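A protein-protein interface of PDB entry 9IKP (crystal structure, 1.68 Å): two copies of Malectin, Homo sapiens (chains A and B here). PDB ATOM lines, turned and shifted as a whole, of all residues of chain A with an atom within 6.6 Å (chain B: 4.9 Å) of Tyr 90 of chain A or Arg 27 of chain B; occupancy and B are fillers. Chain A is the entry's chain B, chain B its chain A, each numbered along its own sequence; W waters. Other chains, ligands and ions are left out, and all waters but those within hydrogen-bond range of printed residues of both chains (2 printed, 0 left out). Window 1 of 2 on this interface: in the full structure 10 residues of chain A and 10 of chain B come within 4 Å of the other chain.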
ATOM      1  N   TYR A  41       2.109  -3.665  22.970  1.00  0.00           N
ATOM      2  CA  TYR A  41       1.273  -2.508  22.632  1.00  0.00           C
ATOM      3  C   TYR A  41       0.376  -2.770  21.418  1.00  0.00           C
ATOM      4  O   TYR A  41      -0.792  -2.357  21.399  1.00  0.00           O
ATOM      5  CB  TYR A  41       2.157  -1.268  22.405  1.00  0.00           C
ATOM      6  CG  TYR A  41       1.363   0.006  22.102  1.00  0.00           C
ATOM      7  CD1 TYR A  41       0.776   0.748  23.120  1.00  0.00           C
ATOM      8  CD2 TYR A  41       1.173   0.443  20.784  1.00  0.00           C
ATOM      9  CE1 TYR A  41       0.017   1.906  22.835  1.00  0.00           C
ATOM     10  CE2 TYR A  41       0.423   1.595  20.492  1.00  0.00           C
ATOM     11  CZ  TYR A  41      -0.148   2.323  21.523  1.00  0.00           C
ATOM     12  OH  TYR A  41      -0.900   3.464  21.231  1.00  0.00           O
ATOM     13  N   LEU A  45      -4.509  -3.575  18.066  1.00  0.00           N
ATOM     14  CA  LEU A  45      -4.676  -3.152  16.673  1.00  0.00           C
ATOM     15  C   LEU A  45      -4.866  -4.328  15.719  1.00  0.00           C
ATOM     16  O   LEU A  45      -4.105  -5.307  15.794  1.00  0.00           O
ATOM     17  CB  LEU A  45      -3.435  -2.334  16.209  1.00  0.00           C
ATOM     18  CG  LEU A  45      -2.921  -1.253  17.164  1.00  0.00           C
ATOM     19  CD1 LEU A  45      -1.682  -0.571  16.608  1.00  0.00           C
ATOM     20  CD2 LEU A  45      -4.020  -0.234  17.413  1.00  0.00           C
ATOM     21  N   ALA A  87       6.261  -4.596  11.817  1.00  0.00           N
ATOM     22  CA  ALA A  87       5.097  -3.711  11.679  1.00  0.00           C
ATOM     23  C   ALA A  87       5.333  -2.429  12.487  1.00  0.00           C
ATOM     24  O   ALA A  87       5.940  -2.463  13.569  1.00  0.00           O
ATOM     25  CB  ALA A  87       3.781  -4.374  12.139  1.00  0.00           C
ATOM     26  N   GLU A  88       4.832  -1.288  11.960  1.00  0.00           N
ATOM     27  CA  GLU A  88       4.903   0.013  12.646  1.00  0.00           C
ATOM     28  C   GLU A  88       3.564   0.255  13.355  1.00  0.00           C
ATOM     29  O   GLU A  88       2.559   0.582  12.715  1.00  0.00           O
ATOM     30  CB  GLU A  88       5.253   1.134  11.661  1.00  0.00           C
ATOM     31  CG  GLU A  88       5.285   2.567  12.281  1.00  0.00           C
ATOM     32  CD  GLU A  88       6.258   2.709  13.439  1.00  0.00           C
ATOM     33  OE1 GLU A  88       7.492   2.740  13.204  1.00  0.00           O
ATOM     34  OE2 GLU A  88       5.770   2.773  14.596  1.00  0.00           O
ATOM     35  N   VAL A  89       3.544   0.083  14.684  1.00  0.00           N
ATOM     36  CA  VAL A  89       2.296   0.186  15.455  1.00  0.00           C
ATOM     37  C   VAL A  89       2.175   1.524  16.210  1.00  0.00           C
ATOM     38  O   VAL A  89       1.249   1.682  17.025  1.00  0.00           O
ATOM     39  CB  VAL A  89       2.124  -1.009  16.429  1.00  0.00           C
ATOM     40  CG1 VAL A  89       2.013  -2.356  15.666  1.00  0.00           C
ATOM     41  CG2 VAL A  89       3.239  -1.043  17.485  1.00  0.00           C
ATOM     42  N   TYR A  90       3.065   2.506  15.946  1.00  0.00           N
ATOM     43  CA  TYR A  90       3.018   3.798  16.654  1.00  0.00           C
ATOM     44  C   TYR A  90       3.008   5.018  15.715  1.00  0.00           C
ATOM     45  O   TYR A  90       2.103   5.861  15.821  1.00  0.00           O
ATOM     46  CB  TYR A  90       4.182   3.900  17.674  1.00  0.00           C
ATOM     47  CG  TYR A  90       4.089   5.065  18.687  1.00  0.00           C
ATOM     48  CD1 TYR A  90       3.263   4.978  19.821  1.00  0.00           C
ATOM     49  CD2 TYR A  90       4.856   6.226  18.530  1.00  0.00           C
ATOM     50  CE1 TYR A  90       3.181   6.050  20.750  1.00  0.00           C
ATOM     51  CE2 TYR A  90       4.779   7.295  19.455  1.00  0.00           C
ATOM     52  CZ  TYR A  90       3.940   7.196  20.553  1.00  0.00           C
ATOM     53  OH  TYR A  90       3.863   8.253  21.467  1.00  0.00           O
ATOM     54  N   PHE A  91       3.990   5.147  14.812  1.00  0.00           N
ATOM     55  CA  PHE A  91       4.113   6.308  13.922  1.00  0.00           C
ATOM     56  C   PHE A  91       3.281   6.164  12.635  1.00  0.00           C
ATOM     57  O   PHE A  91       2.912   5.061  12.216  1.00  0.00           O
ATOM     58  CB  PHE A  91       5.591   6.545  13.563  1.00  0.00           C
ATOM     59  CG  PHE A  91       6.451   6.945  14.743  1.00  0.00           C
ATOM     60  CD1 PHE A  91       6.302   8.199  15.326  1.00  0.00           C
ATOM     61  CD2 PHE A  91       7.384   6.065  15.278  1.00  0.00           C
ATOM     62  CE1 PHE A  91       7.101   8.589  16.399  1.00  0.00           C
ATOM     63  CE2 PHE A  91       8.175   6.433  16.369  1.00  0.00           C
ATOM     64  CZ  PHE A  91       8.030   7.695  16.936  1.00  0.00           C
ATOM     65  N   ALA A  92       2.989   7.322  12.004  1.00  0.00           N
ATOM     66  CA  ALA A  92       2.213   7.421  10.754  1.00  0.00           C
ATOM     67  C   ALA A  92       2.730   8.561   9.853  1.00  0.00           C
ATOM     68  O   ALA A  92       1.954   9.215   9.134  1.00  0.00           O
ATOM     69  CB  ALA A  92       0.717   7.598  11.044  1.00  0.00           C
ATOM     70  N   LYS A  97      10.897   6.653  12.541  1.00  0.00           N
ATOM     71  CA  LYS A  97      11.702   5.508  13.004  1.00  0.00           C
ATOM     72  C   LYS A  97      12.453   4.925  11.805  1.00  0.00           C
ATOM     73  O   LYS A  97      11.816   4.490  10.836  1.00  0.00           O
ATOM     74  CB  LYS A  97      10.814   4.425  13.650  1.00  0.00           C
ATOM     75  CG  LYS A  97      11.572   3.159  14.140  1.00  0.00           C
ATOM     76  CD  LYS A  97      10.648   1.921  14.425  1.00  0.00           C
ATOM     77  CE  LYS A  97       9.679   2.061  15.617  1.00  0.00           C
ATOM     78  NZ  LYS A  97      10.415   2.110  16.943  1.00  0.00           N
ATOM     79  N   HIS A 120       0.794   2.374   8.225  1.00  0.00           N
ATOM     80  CA  HIS A 120       0.564   2.115   9.666  1.00  0.00           C
ATOM     81  C   HIS A 120      -0.129   0.766   9.880  1.00  0.00           C
ATOM     82  O   HIS A 120      -1.036   0.396   9.128  1.00  0.00           O
ATOM     83  CB  HIS A 120      -0.273   3.263  10.281  1.00  0.00           C
ATOM     84  CG  HIS A 120      -0.498   3.181  11.772  1.00  0.00           C
ATOM     85  ND1 HIS A 120       0.510   3.389  12.692  1.00  0.00           N
ATOM     86  CD2 HIS A 120      -1.623   2.957  12.498  1.00  0.00           C
ATOM     87  CE1 HIS A 120       0.021   3.271  13.918  1.00  0.00           C
ATOM     88  NE2 HIS A 120      -1.270   3.012  13.830  1.00  0.00           N
ATOM     89  N   SER A 121       0.328   0.022  10.907  1.00  0.00           N
ATOM     90  CA  SER A 121      -0.326  -1.206  11.387  1.00  0.00           C
ATOM     91  C   SER A 121      -0.524  -2.233  10.258  1.00  0.00           C
ATOM     92  O   SER A 121      -1.594  -2.831  10.109  1.00  0.00           O
ATOM     93  CB  SER A 121      -1.652  -0.855  12.084  1.00  0.00           C
ATOM     94  OG  SER A 121      -2.147  -1.920  12.882  1.00  0.00           O
ATOM     95  N   ASP A 160      14.392   7.459  16.374  1.00  0.00           N
ATOM     96  CA  ASP A 160      13.702   6.539  17.304  1.00  0.00           C
ATOM     97  C   ASP A 160      14.498   5.229  17.448  1.00  0.00           C
ATOM     98  O   ASP A 160      15.726   5.230  17.324  1.00  0.00           O
ATOM     99  CB  ASP A 160      12.244   6.370  16.892  1.00  0.00           C
ATOM    100  CG  ASP A 160      11.350   5.882  18.049  1.00  0.00           C
ATOM    101  OD1 ASP A 160      10.976   6.710  18.933  1.00  0.00           O
ATOM    102  OD2 ASP A 160      10.966   4.677  18.066  1.00  0.00           O
ATOM    103  N   LYS A 163      13.790  -2.261  16.150  1.00  0.00           N
ATOM    104  CA  LYS A 163      12.811  -3.265  16.627  1.00  0.00           C
ATOM    105  C   LYS A 163      12.716  -4.448  15.656  1.00  0.00           C
ATOM    106  O   LYS A 163      13.119  -4.345  14.492  1.00  0.00           O
ATOM    107  CB  LYS A 163      11.403  -2.643  16.817  1.00  0.00           C
ATOM    108  CG  LYS A 163      10.710  -2.260  15.465  1.00  0.00           C
ATOM    109  CD  LYS A 163       9.225  -1.832  15.613  1.00  0.00           C
ATOM    110  CE  LYS A 163       8.258  -3.020  15.738  1.00  0.00           C
ATOM    111  NZ  LYS A 163       6.885  -2.604  16.267  1.00  0.00           N
ATOM    112  N   VAL B   7      -4.782   9.907   8.702  1.00  0.00           N
ATOM    113  CA  VAL B   7      -4.466  10.415  10.045  1.00  0.00           C
ATOM    114  C   VAL B   7      -2.960  10.294  10.300  1.00  0.00           C
ATOM    115  O   VAL B   7      -2.401   9.185  10.257  1.00  0.00           O
ATOM    116  CB  VAL B   7      -5.275   9.670  11.124  1.00  0.00           C
ATOM    117  CG1 VAL B   7      -4.861  10.076  12.538  1.00  0.00           C
ATOM    118  CG2 VAL B   7      -6.792   9.886  10.957  1.00  0.00           C
ATOM    119  N   ALA B  10      -2.455  11.097  16.586  1.00  0.00           N
ATOM    120  CA  ALA B  10      -3.689  11.068  17.392  1.00  0.00           C
ATOM    121  C   ALA B  10      -3.409  10.589  18.825  1.00  0.00           C
ATOM    122  O   ALA B  10      -2.587   9.683  19.018  1.00  0.00           O
ATOM    123  CB  ALA B  10      -4.742  10.152  16.742  1.00  0.00           C
ATOM    124  N   VAL B  11      -4.099  11.195  19.824  1.00  0.00           N
ATOM    125  CA  VAL B  11      -3.851  10.946  21.263  1.00  0.00           C
ATOM    126  C   VAL B  11      -5.165  10.774  22.038  1.00  0.00           C
ATOM    127  O   VAL B  11      -6.094  11.576  21.878  1.00  0.00           O
ATOM    128  CB  VAL B  11      -3.042  12.110  21.895  1.00  0.00           C
ATOM    129  CG1 VAL B  11      -3.029  12.002  23.423  1.00  0.00           C
ATOM    130  CG2 VAL B  11      -1.606  12.146  21.355  1.00  0.00           C
ATOM    131  N   ASN B  12      -5.227   9.749  22.926  1.00  0.00           N
ATOM    132  CA  ASN B  12      -6.275   9.629  23.967  1.00  0.00           C
ATOM    133  C   ASN B  12      -5.737  10.227  25.271  1.00  0.00           C
ATOM    134  O   ASN B  12      -5.030   9.557  26.026  1.00  0.00           O
ATOM    135  CB  ASN B  12      -6.715   8.168  24.167  1.00  0.00           C
ATOM    136  CG  ASN B  12      -7.842   8.025  25.205  1.00  0.00           C
ATOM    137  OD1 ASN B  12      -8.535   9.000  25.503  1.00  0.00           O
ATOM    138  ND2 ASN B  12      -8.021   6.815  25.771  1.00  0.00           N
ATOM    139  N   GLU B  16      -5.344   5.000  27.770  1.00  0.00           N
ATOM    140  CA  GLU B  16      -4.613   3.983  27.009  1.00  0.00           C
ATOM    141  C   GLU B  16      -5.023   4.009  25.530  1.00  0.00           C
ATOM    142  O   GLU B  16      -5.931   4.737  25.129  1.00  0.00           O
ATOM    143  CB  GLU B  16      -4.883   2.599  27.609  1.00  0.00           C
ATOM    144  CG  GLU B  16      -4.563   2.472  29.089  1.00  0.00           C
ATOM    145  CD  GLU B  16      -3.087   2.564  29.391  1.00  0.00           C
ATOM    146  OE1 GLU B  16      -2.731   2.788  30.570  1.00  0.00           O
ATOM    147  OE2 GLU B  16      -2.275   2.354  28.464  1.00  0.00           O
ATOM    148  N   ALA B  17      -4.363   3.179  24.709  1.00  0.00           N
ATOM    149  CA  ALA B  17      -4.707   3.103  23.284  1.00  0.00           C
ATOM    150  C   ALA B  17      -6.167   2.689  23.077  1.00  0.00           C
ATOM    151  O   ALA B  17      -6.706   1.880  23.837  1.00  0.00           O
ATOM    152  CB  ALA B  17      -3.788   2.102  22.579  1.00  0.00           C
ATOM    153  N   HIS B  25      -6.852   5.168  15.296  1.00  0.00           N
ATOM    154  CA  HIS B  25      -6.075   4.716  16.465  1.00  0.00           C
ATOM    155  C   HIS B  25      -5.647   5.934  17.292  1.00  0.00           C
ATOM    156  O   HIS B  25      -4.761   6.692  16.882  1.00  0.00           O
ATOM    157  CB  HIS B  25      -4.869   3.896  15.968  1.00  0.00           C
ATOM    158  CG  HIS B  25      -3.802   3.606  16.993  1.00  0.00           C
ATOM    159  ND1 HIS B  25      -2.523   3.217  16.633  1.00  0.00           N
ATOM    160  CD2 HIS B  25      -3.818   3.619  18.350  1.00  0.00           C
ATOM    161  CE1 HIS B  25      -1.798   3.024  17.725  1.00  0.00           C
ATOM    162  NE2 HIS B  25      -2.558   3.269  18.780  1.00  0.00           N
ATOM    163  N   PHE B  26      -6.288   6.141  18.453  1.00  0.00           N
ATOM    164  CA  PHE B  26      -5.880   7.170  19.414  1.00  0.00           C
ATOM    165  C   PHE B  26      -4.803   6.549  20.313  1.00  0.00           C
ATOM    166  O   PHE B  26      -5.080   5.574  21.021  1.00  0.00           O
ATOM    167  CB  PHE B  26      -7.095   7.679  20.209  1.00  0.00           C
ATOM    168  CG  PHE B  26      -8.085   8.479  19.380  1.00  0.00           C
ATOM    169  CD1 PHE B  26      -9.091   7.845  18.639  1.00  0.00           C
ATOM    170  CD2 PHE B  26      -8.015   9.871  19.362  1.00  0.00           C
ATOM    171  CE1 PHE B  26      -9.992   8.592  17.865  1.00  0.00           C
ATOM    172  CE2 PHE B  26      -8.911  10.631  18.589  1.00  0.00           C
ATOM    173  CZ  PHE B  26      -9.898   9.992  17.842  1.00  0.00           C
ATOM    174  N   ARG B  27      -3.564   7.061  20.240  1.00  0.00           N
ATOM    175  CA  ARG B  27      -2.427   6.459  20.954  1.00  0.00           C
ATOM    176  C   ARG B  27      -2.469   6.724  22.471  1.00  0.00           C
ATOM    177  O   ARG B  27      -3.059   7.700  22.942  1.00  0.00           O
ATOM    178  CB  ARG B  27      -1.091   6.992  20.395  1.00  0.00           C
ATOM    179  CG  ARG B  27      -0.562   6.393  19.047  1.00  0.00           C
ATOM    180  CD  ARG B  27      -1.483   6.616  17.805  1.00  0.00           C
ATOM    181  NE  ARG B  27      -0.731   6.414  16.547  1.00  0.00           N
ATOM    182  CZ  ARG B  27      -1.217   6.634  15.323  1.00  0.00           C
ATOM    183  NH1 ARG B  27      -2.494   6.917  15.119  1.00  0.00           N
ATOM    184  NH2 ARG B  27      -0.399   6.564  14.268  1.00  0.00           N
ATOM    185  N   LYS B  28      -1.823   5.842  23.250  1.00  0.00           N
ATOM    186  CA  LYS B  28      -1.645   6.080  24.692  1.00  0.00           C
ATOM    187  C   LYS B  28      -0.970   7.443  24.910  1.00  0.00           C
ATOM    188  O   LYS B  28      -0.106   7.852  24.129  1.00  0.00           O
ATOM    189  CB  LYS B  28      -0.820   4.903  25.284  1.00  0.00           C
ATOM    190  CG  LYS B  28      -0.358   4.954  26.761  1.00  0.00           C
ATOM    191  CD  LYS B  28      -1.315   5.703  27.644  1.00  0.00           C
ATOM    192  CE  LYS B  28      -1.172   5.549  29.143  1.00  0.00           C
ATOM    193  NZ  LYS B  28      -1.858   6.716  29.799  1.00  0.00           N
ATOM    194  N   ASP B  29      -1.415   8.176  25.945  1.00  0.00           N
ATOM    195  CA  ASP B  29      -1.000   9.576  26.181  1.00  0.00           C
ATOM    196  C   ASP B  29       0.517   9.735  26.353  1.00  0.00           C
ATOM    197  O   ASP B  29       1.083   9.200  27.324  1.00  0.00           O
ATOM    198  CB  ASP B  29      -1.745  10.109  27.422  1.00  0.00           C
ATOM    199  CG  ASP B  29      -1.620  11.637  27.615  1.00  0.00           C
ATOM    200  OD1 ASP B  29      -0.876  12.316  26.867  1.00  0.00           O
ATOM    201  OD2 ASP B  29      -2.311  12.178  28.522  1.00  0.00           O
ATOM    202  N   PRO B  30       1.204  10.470  25.460  1.00  0.00           N
ATOM    203  CA  PRO B  30       2.666  10.652  25.611  1.00  0.00           C
ATOM    204  C   PRO B  30       3.088  11.589  26.749  1.00  0.00           C
ATOM    205  O   PRO B  30       4.294  11.645  27.060  1.00  0.00           O
ATOM    206  CB  PRO B  30       3.093  11.225  24.251  1.00  0.00           C
ATOM    207  CG  PRO B  30       1.866  11.865  23.697  1.00  0.00           C
ATOM    208  CD  PRO B  30       0.712  11.016  24.178  1.00  0.00           C
HETATM  209  O   HOH W   1      -0.555   8.912   7.597  1.00  0.00           O
HETATM  210  O   HOH W   2       2.691   7.721  23.774  1.00  0.00           O
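Of the 13 printed residues of chain A, 6 touch a printed residue of chain B.
Among the printed residues, no Asp or Glu carboxylate lies within 4 Å of a Lys or Arg side-chain nitrogen of the other chain.
The side-chain carboxylate (OE2) of Glu 88 of chain A sits at hydrogen-bond distance from the backbone NH (N) of Tyr 90 of chain A (3.0 Å).
The backbone carbonyl oxygen (O) of Glu 88 of chain A lies within hydrogen-bond range of a ring nitrogen (ND1) of His 120 of chain A (3.5 Å).
O of His 25 of chain B lies within hydrogen-bond range of NH1 of Arg 27 of chain B.
The backbone carbonyl oxygen of Phe 91 of chain A sits at hydrogen-bond distance from a ring nitrogen (ND1) of His 120 of chain A (3.0 Å).
The backbone NH (N) of Asn 12 of chain B sits at hydrogen-bond distance from the backbone carbonyl oxygen (O) of Arg 27 of chain B.
The backbone NH (N) of Arg 27 of chain B sits at hydrogen-bond distance from the backbone carbonyl oxygen (O) of Ala 10 of chain B.
OH of Tyr 41 of chain A touches CB of Ala 17 of chain B, at 3.5 Å.
Tyr 41 of chain A touches Arg 27 of chain B (OH to CA, 3.4 Å).
His 25 of chain B touches Leu 45 of chain A (CE1 to CD1, 3.8 Å).
Val 89 of chain A touches His 25 of chain B (O to CE1, 3.4 Å).
CB of Ala 92 of chain A touches O of Val 7 of chain B, at 3.6 Å.
CB of Ala 92 of chain A touches NH2 of Arg 27 of chain B (3.6 Å).
Arg 27 of chain B touches His 120 of chain A (NH2 to CE1, 3.3 Å).
Of the printed residues of chain B, Tyr 41 of chain A touches Ala 17, His 25, Arg 27 and Lys 28.
Printed residues of chain B within 4 Å of Val 89 of chain A: His 25 (3.4 Å).
Tyr 90 of chain A touches just one residue of chain B: Arg 27 (3.0 Å).
Printed residues of chain A within 4 Å of Val 7 of chain B: Ala 92 (3.6 Å).
Glu 16 of chain B touches none of the printed residues of chain A.
Printed residues of chain A within 4 Å of His 25 of chain B: Tyr 41 (3.0 Å), Leu 45 (3.8 Å), Val 89 (3.4 Å) and His 120 (3.1 Å).
The nearest printed residue of chain B that does not touch Ala 92 of chain A is Ala 10 of chain B (7.3 Å).
No position is printed for both chains.
Water W2 lies within hydrogen-bond range of OH of Tyr 90 of chain A (2.6 Å) and O of Lys 28 of chain B (2.8 Å).
Water W1 lies within hydrogen-bond range of the backbone carbonyl oxygen (O) of Ala 92 of chain A and the backbone carbonyl oxygen (O) of Val 7 of chain B.
NE2 of His 25 of chain B is in hydrogen-bond range of OH of Tyr 41 of chain A (3.0 Å).
A ring nitrogen (NE2) of His 120 of chain A is in hydrogen-bond range of a ring nitrogen (ND1) of His 25 of chain B (3.1 Å).
N of Lys 28 of chain B lies within hydrogen-bond range of OH of Tyr 41 of chain A (3.3 Å).
The guanidinium group (NE) of Arg 27 of chain B is in hydrogen-bond range of the backbone carbonyl oxygen (O) of Tyr 90 of chain A (3.0 Å).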
